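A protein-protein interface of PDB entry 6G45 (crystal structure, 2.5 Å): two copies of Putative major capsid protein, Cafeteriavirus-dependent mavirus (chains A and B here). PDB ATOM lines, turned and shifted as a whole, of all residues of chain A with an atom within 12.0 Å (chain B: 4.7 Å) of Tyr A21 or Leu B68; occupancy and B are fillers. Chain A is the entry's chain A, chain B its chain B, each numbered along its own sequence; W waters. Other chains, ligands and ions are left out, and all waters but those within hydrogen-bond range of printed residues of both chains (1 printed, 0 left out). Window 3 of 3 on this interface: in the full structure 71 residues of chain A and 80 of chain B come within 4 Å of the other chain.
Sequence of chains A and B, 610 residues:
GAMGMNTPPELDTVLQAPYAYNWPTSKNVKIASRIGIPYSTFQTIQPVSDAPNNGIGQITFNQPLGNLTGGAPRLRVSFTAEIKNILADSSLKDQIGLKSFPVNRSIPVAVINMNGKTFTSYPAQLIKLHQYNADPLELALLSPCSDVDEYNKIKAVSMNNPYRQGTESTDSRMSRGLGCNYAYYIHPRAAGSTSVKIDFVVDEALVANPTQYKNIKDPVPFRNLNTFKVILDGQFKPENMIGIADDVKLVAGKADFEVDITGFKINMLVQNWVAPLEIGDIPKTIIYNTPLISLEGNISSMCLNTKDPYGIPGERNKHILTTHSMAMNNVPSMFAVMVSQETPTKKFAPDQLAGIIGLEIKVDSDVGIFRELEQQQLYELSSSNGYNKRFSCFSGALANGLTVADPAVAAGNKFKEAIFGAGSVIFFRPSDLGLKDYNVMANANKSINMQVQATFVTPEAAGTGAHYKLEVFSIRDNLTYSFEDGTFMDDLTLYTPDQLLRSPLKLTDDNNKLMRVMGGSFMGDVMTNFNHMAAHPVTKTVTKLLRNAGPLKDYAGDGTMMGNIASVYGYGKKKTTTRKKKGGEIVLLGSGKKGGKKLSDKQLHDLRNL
The side-chain hydroxyl of Tyr A21 lies within hydrogen-bond range of the indole nitrogen of Trp B273, 2.8 Å away.
O of Trp B273 sits at hydrogen-bond distance from N of Leu B68, 3.0 Å away.
O of Leu B68 lies within hydrogen-bond range of ND2 of Asn B272 (3.0 Å).
O of Trp A23 lies within hydrogen-bond range of ND2 of Asn A28 (3.1 Å).
O of Tyr A21 sits close to NE1 of Trp A23 (3.3 Å).
CA of Gly B36 touches CG of Pro A18 (3.8 Å).
Pro A18 touches Ile B37 (CG to N, 3.9 Å).
Ala A20 touches Pro B221.
Ile B37 touches Tyr A21.
Leu B68 touches Tyr A21 (CD1 to CE1, 3.9 Å).
Tyr A21 touches Pro B276.
CD2 of Tyr A21 touches CG2 of Ile B279 (3.8 Å).
Pro B221 touches Trp A23.
Of the printed residues of chain B, Pro A18 touches Gly B36 and Ile B37.
Of the printed residues of chain B, Ala A20 touches Pro B221.
Of chain B, only Ile B37, Leu B68, Trp B273, Pro B276 and Ile B279 come within 4 Å of Tyr A21.
Of the printed residues of chain B, Trp A23 touches Pro B221 (3.7 Å).
Thr A25 touches none of the printed residues of chain B.
Val A29 touches none of the printed residues of chain B.
Of the printed residues of chain A, Gly B36 touches Pro A18.
No residue of chain A comes within 4 Å of Gly B66.
Asn B67 touches none of the printed residues of chain A.
Of the printed residues of chain A, Leu B68 touches Tyr A21 (3.9 Å).
No residue of chain A comes within 4 Å of Thr B69.
No residue of chain A comes within 4 Å of Gly B70.
Of chain A, only Ala A20 and Trp A23 come within 4 Å of Pro B221.
No residue of chain A comes within 4 Å of Asn B272.
Of the printed residues of chain A, Trp B273 touches Tyr A21.
No residue of chain A comes within 4 Å of Ala B275.
Printed residues of chain A within 4 Å of Pro B276: Tyr A21.
Ile B279 touches one residue of chain A.
The nearest residue of chain A that does not touch Leu B68 is Trp A23 (4.1 Å).
The nearest printed residue of chain B that does not touch Ala A20 is Ile B37 (4.1 Å).
Of the 14 printed residues of chain A, 4 touch a printed residue of chain B.
Printed residues of chain A that touch a printed residue of chain B: Pro A18, Ala A20, Tyr A21 and Trp A23.
Hydrophobic or aromatic side chains of chain A within 4 Å of the printed part of chain B: Pro A18, Tyr A21 and Trp A23.
Of the 17 printed residues of chain B, 7 touch a printed residue of chain A.
Hydrophobic or aromatic side chains of chain B within 4 Å of the printed part of chain A: Ile B37, Leu B68, Pro B221, Trp B273, Pro B276 and Ile B279.
Among the printed residues, 9 pairs touch across the chains.
No position is printed for both chains.
Of the 9 pairs that touch across the chains among the printed residues, none has its exchanged pair printed and touching as well.
Water W1 bridges OH of Tyr A21 (2.7 Å) and O of Gly B36 (2.7 Å).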
ATOM      1  N   LEU A  15      21.278 -24.438 -24.160  1.00  0.00           N
ATOM      2  CA  LEU A  15      21.045 -23.908 -22.823  1.00  0.00           C
ATOM      3  C   LEU A  15      22.338 -24.052 -22.035  1.00  0.00           C
ATOM      4  O   LEU A  15      22.763 -25.169 -21.738  1.00  0.00           O
ATOM      5  CB  LEU A  15      19.905 -24.669 -22.145  1.00  0.00           C
ATOM      6  CG  LEU A  15      19.463 -24.196 -20.757  1.00  0.00           C
ATOM      7  CD1 LEU A  15      18.995 -22.748 -20.770  1.00  0.00           C
ATOM      8  CD2 LEU A  15      18.360 -25.100 -20.227  1.00  0.00           C
ATOM      9  N   GLN A  16      22.977 -22.925 -21.728  1.00  0.00           N
ATOM     10  CA  GLN A  16      24.192 -22.919 -20.915  1.00  0.00           C
ATOM     11  C   GLN A  16      23.853 -22.914 -19.422  1.00  0.00           C
ATOM     12  O   GLN A  16      22.866 -22.313 -19.002  1.00  0.00           O
ATOM     13  CB  GLN A  16      25.070 -21.719 -21.267  1.00  0.00           C
ATOM     14  CG  GLN A  16      25.767 -21.851 -22.615  1.00  0.00           C
ATOM     15  CD  GLN A  16      26.785 -20.753 -22.869  1.00  0.00           C
ATOM     16  OE1 GLN A  16      26.779 -19.712 -22.212  1.00  0.00           O
ATOM     17  NE2 GLN A  16      27.665 -20.981 -23.833  1.00  0.00           N
ATOM     18  N   ALA A  17      24.678 -23.601 -18.635  1.00  0.00           N
ATOM     19  CA  ALA A  17      24.512 -23.670 -17.184  1.00  0.00           C
ATOM     20  C   ALA A  17      25.885 -23.697 -16.511  1.00  0.00           C
ATOM     21  O   ALA A  17      26.877 -24.009 -17.168  1.00  0.00           O
ATOM     22  CB  ALA A  17      23.702 -24.899 -16.803  1.00  0.00           C
ATOM     23  N   PRO A  18      25.952 -23.363 -15.204  1.00  0.00           N
ATOM     24  CA  PRO A  18      27.254 -23.327 -14.530  1.00  0.00           C
ATOM     25  C   PRO A  18      27.955 -24.683 -14.428  1.00  0.00           C
ATOM     26  O   PRO A  18      27.298 -25.730 -14.397  1.00  0.00           O
ATOM     27  CB  PRO A  18      26.921 -22.809 -13.124  1.00  0.00           C
ATOM     28  CG  PRO A  18      25.595 -22.158 -13.238  1.00  0.00           C
ATOM     29  CD  PRO A  18      24.870 -22.880 -14.327  1.00  0.00           C
ATOM     30  N   TYR A  19      29.283 -24.638 -14.363  1.00  0.00           N
ATOM     31  CA  TYR A  19      30.109 -25.826 -14.163  1.00  0.00           C
ATOM     32  C   TYR A  19      29.885 -26.480 -12.792  1.00  0.00           C
ATOM     33  O   TYR A  19      30.168 -27.664 -12.625  1.00  0.00           O
ATOM     34  CB  TYR A  19      31.590 -25.468 -14.346  1.00  0.00           C
ATOM     35  CG  TYR A  19      32.500 -26.668 -14.504  1.00  0.00           C
ATOM     36  CD1 TYR A  19      32.622 -27.317 -15.736  1.00  0.00           C
ATOM     37  CD2 TYR A  19      33.238 -27.159 -13.422  1.00  0.00           C
ATOM     38  CE1 TYR A  19      33.456 -28.421 -15.885  1.00  0.00           C
ATOM     39  CE2 TYR A  19      34.074 -28.261 -13.559  1.00  0.00           C
ATOM     40  CZ  TYR A  19      34.180 -28.889 -14.791  1.00  0.00           C
ATOM     41  OH  TYR A  19      35.008 -29.979 -14.932  1.00  0.00           O
ATOM     42  N   ALA A  20      29.379 -25.713 -11.826  1.00  0.00           N
ATOM     43  CA  ALA A  20      28.982 -26.232 -10.509  1.00  0.00           C
ATOM     44  C   ALA A  20      27.976 -27.390 -10.555  1.00  0.00           C
ATOM     45  O   ALA A  20      27.996 -28.255  -9.676  1.00  0.00           O
ATOM     46  CB  ALA A  20      28.427 -25.102  -9.658  1.00  0.00           C
ATOM     47  N   TYR A  21      27.097 -27.397 -11.560  1.00  0.00           N
ATOM     48  CA  TYR A  21      26.142 -28.496 -11.755  1.00  0.00           C
ATOM     49  C   TYR A  21      26.720 -29.729 -12.464  1.00  0.00           C
ATOM     50  O   TYR A  21      26.014 -30.724 -12.635  1.00  0.00           O
ATOM     51  CB  TYR A  21      24.903 -28.003 -12.514  1.00  0.00           C
ATOM     52  CG  TYR A  21      24.089 -26.938 -11.799  1.00  0.00           C
ATOM     53  CD1 TYR A  21      23.767 -27.052 -10.441  1.00  0.00           C
ATOM     54  CD2 TYR A  21      23.608 -25.829 -12.493  1.00  0.00           C
ATOM     55  CE1 TYR A  21      23.010 -26.082  -9.799  1.00  0.00           C
ATOM     56  CE2 TYR A  21      22.849 -24.856 -11.858  1.00  0.00           C
ATOM     57  CZ  TYR A  21      22.552 -24.989 -10.513  1.00  0.00           C
ATOM     58  OH  TYR A  21      21.801 -24.029  -9.882  1.00  0.00           O
ATOM     59  N   ASN A  22      27.981 -29.664 -12.895  1.00  0.00           N
ATOM     60  CA  ASN A  22      28.703 -30.847 -13.370  1.00  0.00           C
ATOM     61  C   ASN A  22      29.145 -31.644 -12.142  1.00  0.00           C
ATOM     62  O   ASN A  22      30.292 -31.546 -11.694  1.00  0.00           O
ATOM     63  CB  ASN A  22      29.900 -30.442 -14.243  1.00  0.00           C
ATOM     64  CG  ASN A  22      30.557 -31.630 -14.926  1.00  0.00           C
ATOM     65  OD1 ASN A  22      29.877 -32.497 -15.480  1.00  0.00           O
ATOM     66  ND2 ASN A  22      31.887 -31.670 -14.897  1.00  0.00           N
ATOM     67  N   TRP A  23      28.209 -32.424 -11.605  1.00  0.00           N
ATOM     68  CA  TRP A  23      28.372 -33.078 -10.305  1.00  0.00           C
ATOM     69  C   TRP A  23      29.504 -34.106 -10.369  1.00  0.00           C
ATOM     70  O   TRP A  23      29.475 -34.982 -11.233  1.00  0.00           O
ATOM     71  CB  TRP A  23      27.075 -33.781  -9.880  1.00  0.00           C
ATOM     72  CG  TRP A  23      25.851 -32.904  -9.862  1.00  0.00           C
ATOM     73  CD1 TRP A  23      24.856 -32.875 -10.792  1.00  0.00           C
ATOM     74  CD2 TRP A  23      25.494 -31.937  -8.864  1.00  0.00           C
ATOM     75  NE1 TRP A  23      23.903 -31.948 -10.445  1.00  0.00           N
ATOM     76  CE2 TRP A  23      24.268 -31.357  -9.265  1.00  0.00           C
ATOM     77  CE3 TRP A  23      26.091 -31.498  -7.673  1.00  0.00           C
ATOM     78  CZ2 TRP A  23      23.625 -30.368  -8.515  1.00  0.00           C
ATOM     79  CZ3 TRP A  23      25.449 -30.509  -6.925  1.00  0.00           C
ATOM     80  CH2 TRP A  23      24.228 -29.958  -7.351  1.00  0.00           C
ATOM     81  N   PRO A  24      30.517 -33.990  -9.483  1.00  0.00           N
ATOM     82  CA  PRO A  24      31.514 -35.064  -9.424  1.00  0.00           C
ATOM     83  C   PRO A  24      30.913 -36.351  -8.851  1.00  0.00           C
ATOM     84  O   PRO A  24      30.325 -36.325  -7.771  1.00  0.00           O
ATOM     85  CB  PRO A  24      32.613 -34.503  -8.508  1.00  0.00           C
ATOM     86  CG  PRO A  24      32.358 -33.044  -8.409  1.00  0.00           C
ATOM     87  CD  PRO A  24      30.887 -32.857  -8.616  1.00  0.00           C
ATOM     88  N   THR A  25      31.043 -37.447  -9.597  1.00  0.00           N
ATOM     89  CA  THR A  25      30.503 -38.755  -9.218  1.00  0.00           C
ATOM     90  C   THR A  25      31.525 -39.831  -9.580  1.00  0.00           C
ATOM     91  O   THR A  25      32.592 -39.526 -10.115  1.00  0.00           O
ATOM     92  CB  THR A  25      29.170 -39.055  -9.949  1.00  0.00           C
ATOM     93  OG1 THR A  25      29.400 -39.169 -11.357  1.00  0.00           O
ATOM     94  CG2 THR A  25      28.142 -37.962  -9.697  1.00  0.00           C
ATOM     95  N   LYS A  27      31.252 -41.854 -11.964  1.00  0.00           N
ATOM     96  CA  LYS A  27      31.318 -41.888 -13.421  1.00  0.00           C
ATOM     97  C   LYS A  27      32.322 -40.909 -14.045  1.00  0.00           C
ATOM     98  O   LYS A  27      32.781 -41.153 -15.158  1.00  0.00           O
ATOM     99  CB  LYS A  27      29.921 -41.644 -14.000  1.00  0.00           C
ATOM    100  CG  LYS A  27      28.903 -42.695 -13.573  1.00  0.00           C
ATOM    101  CD  LYS A  27      27.572 -42.532 -14.290  1.00  0.00           C
ATOM    102  CE  LYS A  27      26.566 -43.572 -13.820  1.00  0.00           C
ATOM    103  NZ  LYS A  27      25.312 -43.543 -14.623  1.00  0.00           N
ATOM    104  N   ASN A  28      32.654 -39.816 -13.351  1.00  0.00           N
ATOM    105  CA  ASN A  28      33.566 -38.785 -13.897  1.00  0.00           C
ATOM    106  C   ASN A  28      34.739 -38.347 -12.995  1.00  0.00           C
ATOM    107  O   ASN A  28      35.430 -37.380 -13.322  1.00  0.00           O
ATOM    108  CB  ASN A  28      32.754 -37.557 -14.366  1.00  0.00           C
ATOM    109  CG  ASN A  28      32.057 -36.816 -13.226  1.00  0.00           C
ATOM    110  OD1 ASN A  28      32.270 -37.094 -12.047  1.00  0.00           O
ATOM    111  ND2 ASN A  28      31.215 -35.857 -13.586  1.00  0.00           N
ATOM    112  N   VAL A  29      34.964 -39.049 -11.883  1.00  0.00           N
ATOM    113  CA  VAL A  29      36.090 -38.766 -10.984  1.00  0.00           C
ATOM    114  C   VAL A  29      37.044 -39.955 -10.981  1.00  0.00           C
ATOM    115  O   VAL A  29      36.610 -41.107 -10.918  1.00  0.00           O
ATOM    116  CB  VAL A  29      35.627 -38.470  -9.538  1.00  0.00           C
ATOM    117  CG1 VAL A  29      36.820 -38.302  -8.600  1.00  0.00           C
ATOM    118  CG2 VAL A  29      34.774 -37.211  -9.495  1.00  0.00           C
ATOM    119  N   GLY B  36      21.639 -19.853 -14.395  1.00  0.00           N
ATOM    120  CA  GLY B  36      22.780 -19.652 -13.507  1.00  0.00           C
ATOM    121  C   GLY B  36      22.373 -19.770 -12.057  1.00  0.00           C
ATOM    122  O   GLY B  36      21.190 -19.927 -11.748  1.00  0.00           O
ATOM    123  N   ILE B  37      23.367 -19.723 -11.174  1.00  0.00           N
ATOM    124  CA  ILE B  37      23.131 -19.617  -9.742  1.00  0.00           C
ATOM    125  C   ILE B  37      22.785 -18.149  -9.484  1.00  0.00           C
ATOM    126  O   ILE B  37      23.664 -17.297  -9.599  1.00  0.00           O
ATOM    127  CB  ILE B  37      24.365 -20.048  -8.924  1.00  0.00           C
ATOM    128  CG1 ILE B  37      24.692 -21.519  -9.200  1.00  0.00           C
ATOM    129  CG2 ILE B  37      24.120 -19.852  -7.429  1.00  0.00           C
ATOM    130  CD1 ILE B  37      26.033 -21.968  -8.657  1.00  0.00           C
ATOM    131  N   GLY B  66      17.391 -26.162   3.349  1.00  0.00           N
ATOM    132  CA  GLY B  66      16.858 -27.071   2.335  1.00  0.00           C
ATOM    133  C   GLY B  66      17.466 -26.820   0.969  1.00  0.00           C
ATOM    134  O   GLY B  66      18.162 -25.821   0.764  1.00  0.00           O
ATOM    135  N   ASN B  67      17.198 -27.738   0.040  1.00  0.00           N
ATOM    136  CA  ASN B  67      17.637 -27.631  -1.358  1.00  0.00           C
ATOM    137  C   ASN B  67      19.163 -27.464  -1.448  1.00  0.00           C
ATOM    138  O   ASN B  67      19.871 -28.148  -0.713  1.00  0.00           O
ATOM    139  CB  ASN B  67      16.854 -26.531  -2.081  1.00  0.00           C
ATOM    140  CG  ASN B  67      15.366 -26.777  -2.058  1.00  0.00           C
ATOM    141  OD1 ASN B  67      14.616 -26.042  -1.420  1.00  0.00           O
ATOM    142  ND2 ASN B  67      14.931 -27.817  -2.752  1.00  0.00           N
ATOM    143  N   LEU B  68      19.670 -26.575  -2.308  1.00  0.00           N
ATOM    144  CA  LEU B  68      21.112 -26.431  -2.528  1.00  0.00           C
ATOM    145  C   LEU B  68      21.689 -25.279  -1.721  1.00  0.00           C
ATOM    146  O   LEU B  68      21.093 -24.208  -1.667  1.00  0.00           O
ATOM    147  CB  LEU B  68      21.407 -26.196  -4.010  1.00  0.00           C
ATOM    148  CG  LEU B  68      20.900 -27.259  -4.983  1.00  0.00           C
ATOM    149  CD1 LEU B  68      21.268 -26.858  -6.403  1.00  0.00           C
ATOM    150  CD2 LEU B  68      21.460 -28.635  -4.649  1.00  0.00           C
ATOM    151  N   THR B  69      22.850 -25.508  -1.107  1.00  0.00           N
ATOM    152  CA  THR B  69      23.585 -24.481  -0.361  1.00  0.00           C
ATOM    153  C   THR B  69      24.953 -24.297  -1.010  1.00  0.00           C
ATOM    154  O   THR B  69      25.601 -25.277  -1.381  1.00  0.00           O
ATOM    155  CB  THR B  69      23.751 -24.867   1.124  1.00  0.00           C
ATOM    156  OG1 THR B  69      22.459 -24.966   1.733  1.00  0.00           O
ATOM    157  CG2 THR B  69      24.578 -23.823   1.892  1.00  0.00           C
ATOM    158  N   GLY B  70      25.385 -23.039  -1.128  1.00  0.00           N
ATOM    159  CA  GLY B  70      26.640 -22.694  -1.803  1.00  0.00           C
ATOM    160  C   GLY B  70      27.843 -23.344  -1.142  1.00  0.00           C
ATOM    161  O   GLY B  70      27.955 -23.344   0.084  1.00  0.00           O
ATOM    162  N   PRO B 221      27.700 -27.054  -5.024  1.00  0.00           N
ATOM    163  CA  PRO B 221      26.891 -26.860  -3.821  1.00  0.00           C
ATOM    164  C   PRO B 221      26.578 -28.152  -3.077  1.00  0.00           C
ATOM    165  O   PRO B 221      26.610 -29.234  -3.666  1.00  0.00           O
ATOM    166  CB  PRO B 221      25.599 -26.252  -4.369  1.00  0.00           C
ATOM    167  CG  PRO B 221      25.475 -26.836  -5.726  1.00  0.00           C
ATOM    168  CD  PRO B 221      26.880 -26.961  -6.247  1.00  0.00           C
ATOM    169  N   PHE B 222      26.288 -28.011  -1.785  1.00  0.00           N
ATOM    170  CA  PHE B 222      25.779 -29.097  -0.949  1.00  0.00           C
ATOM    171  C   PHE B 222      24.262 -29.117  -1.032  1.00  0.00           C
ATOM    172  O   PHE B 222      23.647 -28.100  -1.355  1.00  0.00           O
ATOM    173  CB  PHE B 222      26.213 -28.893   0.499  1.00  0.00           C
ATOM    174  CG  PHE B 222      27.698 -28.848   0.675  1.00  0.00           C
ATOM    175  CD1 PHE B 222      28.441 -30.020   0.678  1.00  0.00           C
ATOM    176  CD2 PHE B 222      28.361 -27.633   0.811  1.00  0.00           C
ATOM    177  CE1 PHE B 222      29.818 -29.983   0.828  1.00  0.00           C
ATOM    178  CE2 PHE B 222      29.737 -27.589   0.960  1.00  0.00           C
ATOM    179  CZ  PHE B 222      30.466 -28.766   0.971  1.00  0.00           C
ATOM    180  N   ARG B 223      23.664 -30.267  -0.728  1.00  0.00           N
ATOM    181  CA  ARG B 223      22.207 -30.434  -0.838  1.00  0.00           C
ATOM    182  C   ARG B 223      21.558 -30.979   0.433  1.00  0.00           C
ATOM    183  O   ARG B 223      22.121 -31.843   1.109  1.00  0.00           O
ATOM    184  CB  ARG B 223      21.850 -31.345  -2.013  1.00  0.00           C
ATOM    185  CG  ARG B 223      22.576 -32.669  -1.984  1.00  0.00           C
ATOM    186  CD  ARG B 223      21.757 -33.807  -2.544  1.00  0.00           C
ATOM    187  NE  ARG B 223      22.541 -35.022  -2.366  1.00  0.00           N
ATOM    188  CZ  ARG B 223      22.551 -36.074  -3.177  1.00  0.00           C
ATOM    189  NH1 ARG B 223      21.798 -36.124  -4.272  1.00  0.00           N
ATOM    190  NH2 ARG B 223      23.340 -37.092  -2.877  1.00  0.00           N
ATOM    191  N   GLN B 271      24.694 -18.885   0.144  1.00  0.00           N
ATOM    192  CA  GLN B 271      23.707 -18.890  -0.935  1.00  0.00           C
ATOM    193  C   GLN B 271      22.842 -20.135  -0.778  1.00  0.00           C
ATOM    194  O   GLN B 271      23.369 -21.230  -0.566  1.00  0.00           O
ATOM    195  CB  GLN B 271      24.397 -18.913  -2.300  1.00  0.00           C
ATOM    196  CG  GLN B 271      24.889 -17.558  -2.773  1.00  0.00           C
ATOM    197  CD  GLN B 271      25.706 -17.655  -4.047  1.00  0.00           C
ATOM    198  OE1 GLN B 271      26.772 -18.276  -4.072  1.00  0.00           O
ATOM    199  NE2 GLN B 271      25.215 -17.035  -5.111  1.00  0.00           N
ATOM    200  N   ASN B 272      21.525 -19.964  -0.879  1.00  0.00           N
ATOM    201  CA  ASN B 272      20.574 -21.070  -0.781  1.00  0.00           C
ATOM    202  C   ASN B 272      19.534 -20.926  -1.886  1.00  0.00           C
ATOM    203  O   ASN B 272      18.925 -19.866  -2.020  1.00  0.00           O
ATOM    204  CB  ASN B 272      19.902 -21.072   0.596  1.00  0.00           C
ATOM    205  CG  ASN B 272      18.978 -22.260   0.800  1.00  0.00           C
ATOM    206  OD1 ASN B 272      17.768 -22.098   0.932  1.00  0.00           O
ATOM    207  ND2 ASN B 272      19.544 -23.460   0.822  1.00  0.00           N
ATOM    208  N   TRP B 273      19.337 -21.986  -2.672  1.00  0.00           N
ATOM    209  CA  TRP B 273      18.415 -21.952  -3.811  1.00  0.00           C
ATOM    210  C   TRP B 273      17.945 -23.339  -4.251  1.00  0.00           C
ATOM    211  O   TRP B 273      18.570 -24.359  -3.940  1.00  0.00           O
ATOM    212  CB  TRP B 273      19.060 -21.219  -4.998  1.00  0.00           C
ATOM    213  CG  TRP B 273      20.124 -22.006  -5.720  1.00  0.00           C
ATOM    214  CD1 TRP B 273      19.969 -22.718  -6.870  1.00  0.00           C
ATOM    215  CD2 TRP B 273      21.495 -22.161  -5.334  1.00  0.00           C
ATOM    216  NE1 TRP B 273      21.152 -23.311  -7.228  1.00  0.00           N
ATOM    217  CE2 TRP B 273      22.109 -22.985  -6.306  1.00  0.00           C
ATOM    218  CE3 TRP B 273      22.265 -21.687  -4.262  1.00  0.00           C
ATOM    219  CZ2 TRP B 273      23.462 -23.344  -6.242  1.00  0.00           C
ATOM    220  CZ3 TRP B 273      23.616 -22.045  -4.197  1.00  0.00           C
ATOM    221  CH2 TRP B 273      24.197 -22.866  -5.185  1.00  0.00           C
ATOM    222  N   ALA B 275      17.259 -26.203  -6.961  1.00  0.00           N
ATOM    223  CA  ALA B 275      17.878 -26.705  -8.181  1.00  0.00           C
ATOM    224  C   ALA B 275      16.910 -26.549  -9.354  1.00  0.00           C
ATOM    225  O   ALA B 275      15.720 -26.840  -9.207  1.00  0.00           O
ATOM    226  CB  ALA B 275      18.270 -28.165  -8.017  1.00  0.00           C
ATOM    227  N   PRO B 276      17.407 -26.075 -10.513  1.00  0.00           N
ATOM    228  CA  PRO B 276      16.522 -25.910 -11.661  1.00  0.00           C
ATOM    229  C   PRO B 276      16.184 -27.260 -12.290  1.00  0.00           C
ATOM    230  O   PRO B 276      16.986 -28.190 -12.224  1.00  0.00           O
ATOM    231  CB  PRO B 276      17.349 -25.047 -12.611  1.00  0.00           C
ATOM    232  CG  PRO B 276      18.758 -25.433 -12.322  1.00  0.00           C
ATOM    233  CD  PRO B 276      18.812 -25.782 -10.860  1.00  0.00           C
ATOM    234  N   ILE B 279      18.584 -29.056 -15.414  1.00  0.00           N
ATOM    235  CA  ILE B 279      19.777 -29.900 -15.192  1.00  0.00           C
ATOM    236  C   ILE B 279      19.465 -31.387 -14.952  1.00  0.00           C
ATOM    237  O   ILE B 279      20.382 -32.209 -14.916  1.00  0.00           O
ATOM    238  CB  ILE B 279      20.697 -29.368 -14.061  1.00  0.00           C
ATOM    239  CG1 ILE B 279      20.009 -29.388 -12.688  1.00  0.00           C
ATOM    240  CG2 ILE B 279      21.176 -27.962 -14.395  1.00  0.00           C
ATOM    241  CD1 ILE B 279      20.982 -29.399 -11.529  1.00  0.00           C
ATOM    242  N   ILE B 282      19.482 -34.877  -9.858  1.00  0.00           N
ATOM    243  CA  ILE B 282      20.741 -34.781  -9.136  1.00  0.00           C
ATOM    244  C   ILE B 282      21.182 -36.219  -8.820  1.00  0.00           C
ATOM    245  O   ILE B 282      20.355 -37.017  -8.377  1.00  0.00           O
ATOM    246  CB  ILE B 282      20.583 -33.938  -7.851  1.00  0.00           C
ATOM    247  CG1 ILE B 282      20.169 -32.504  -8.220  1.00  0.00           C
ATOM    248  CG2 ILE B 282      21.881 -33.913  -7.048  1.00  0.00           C
ATOM    249  CD1 ILE B 282      19.679 -31.671  -7.055  1.00  0.00           C
HETATM  250  O   HOH W   1      20.281 -22.434 -11.362  1.00  0.00           O
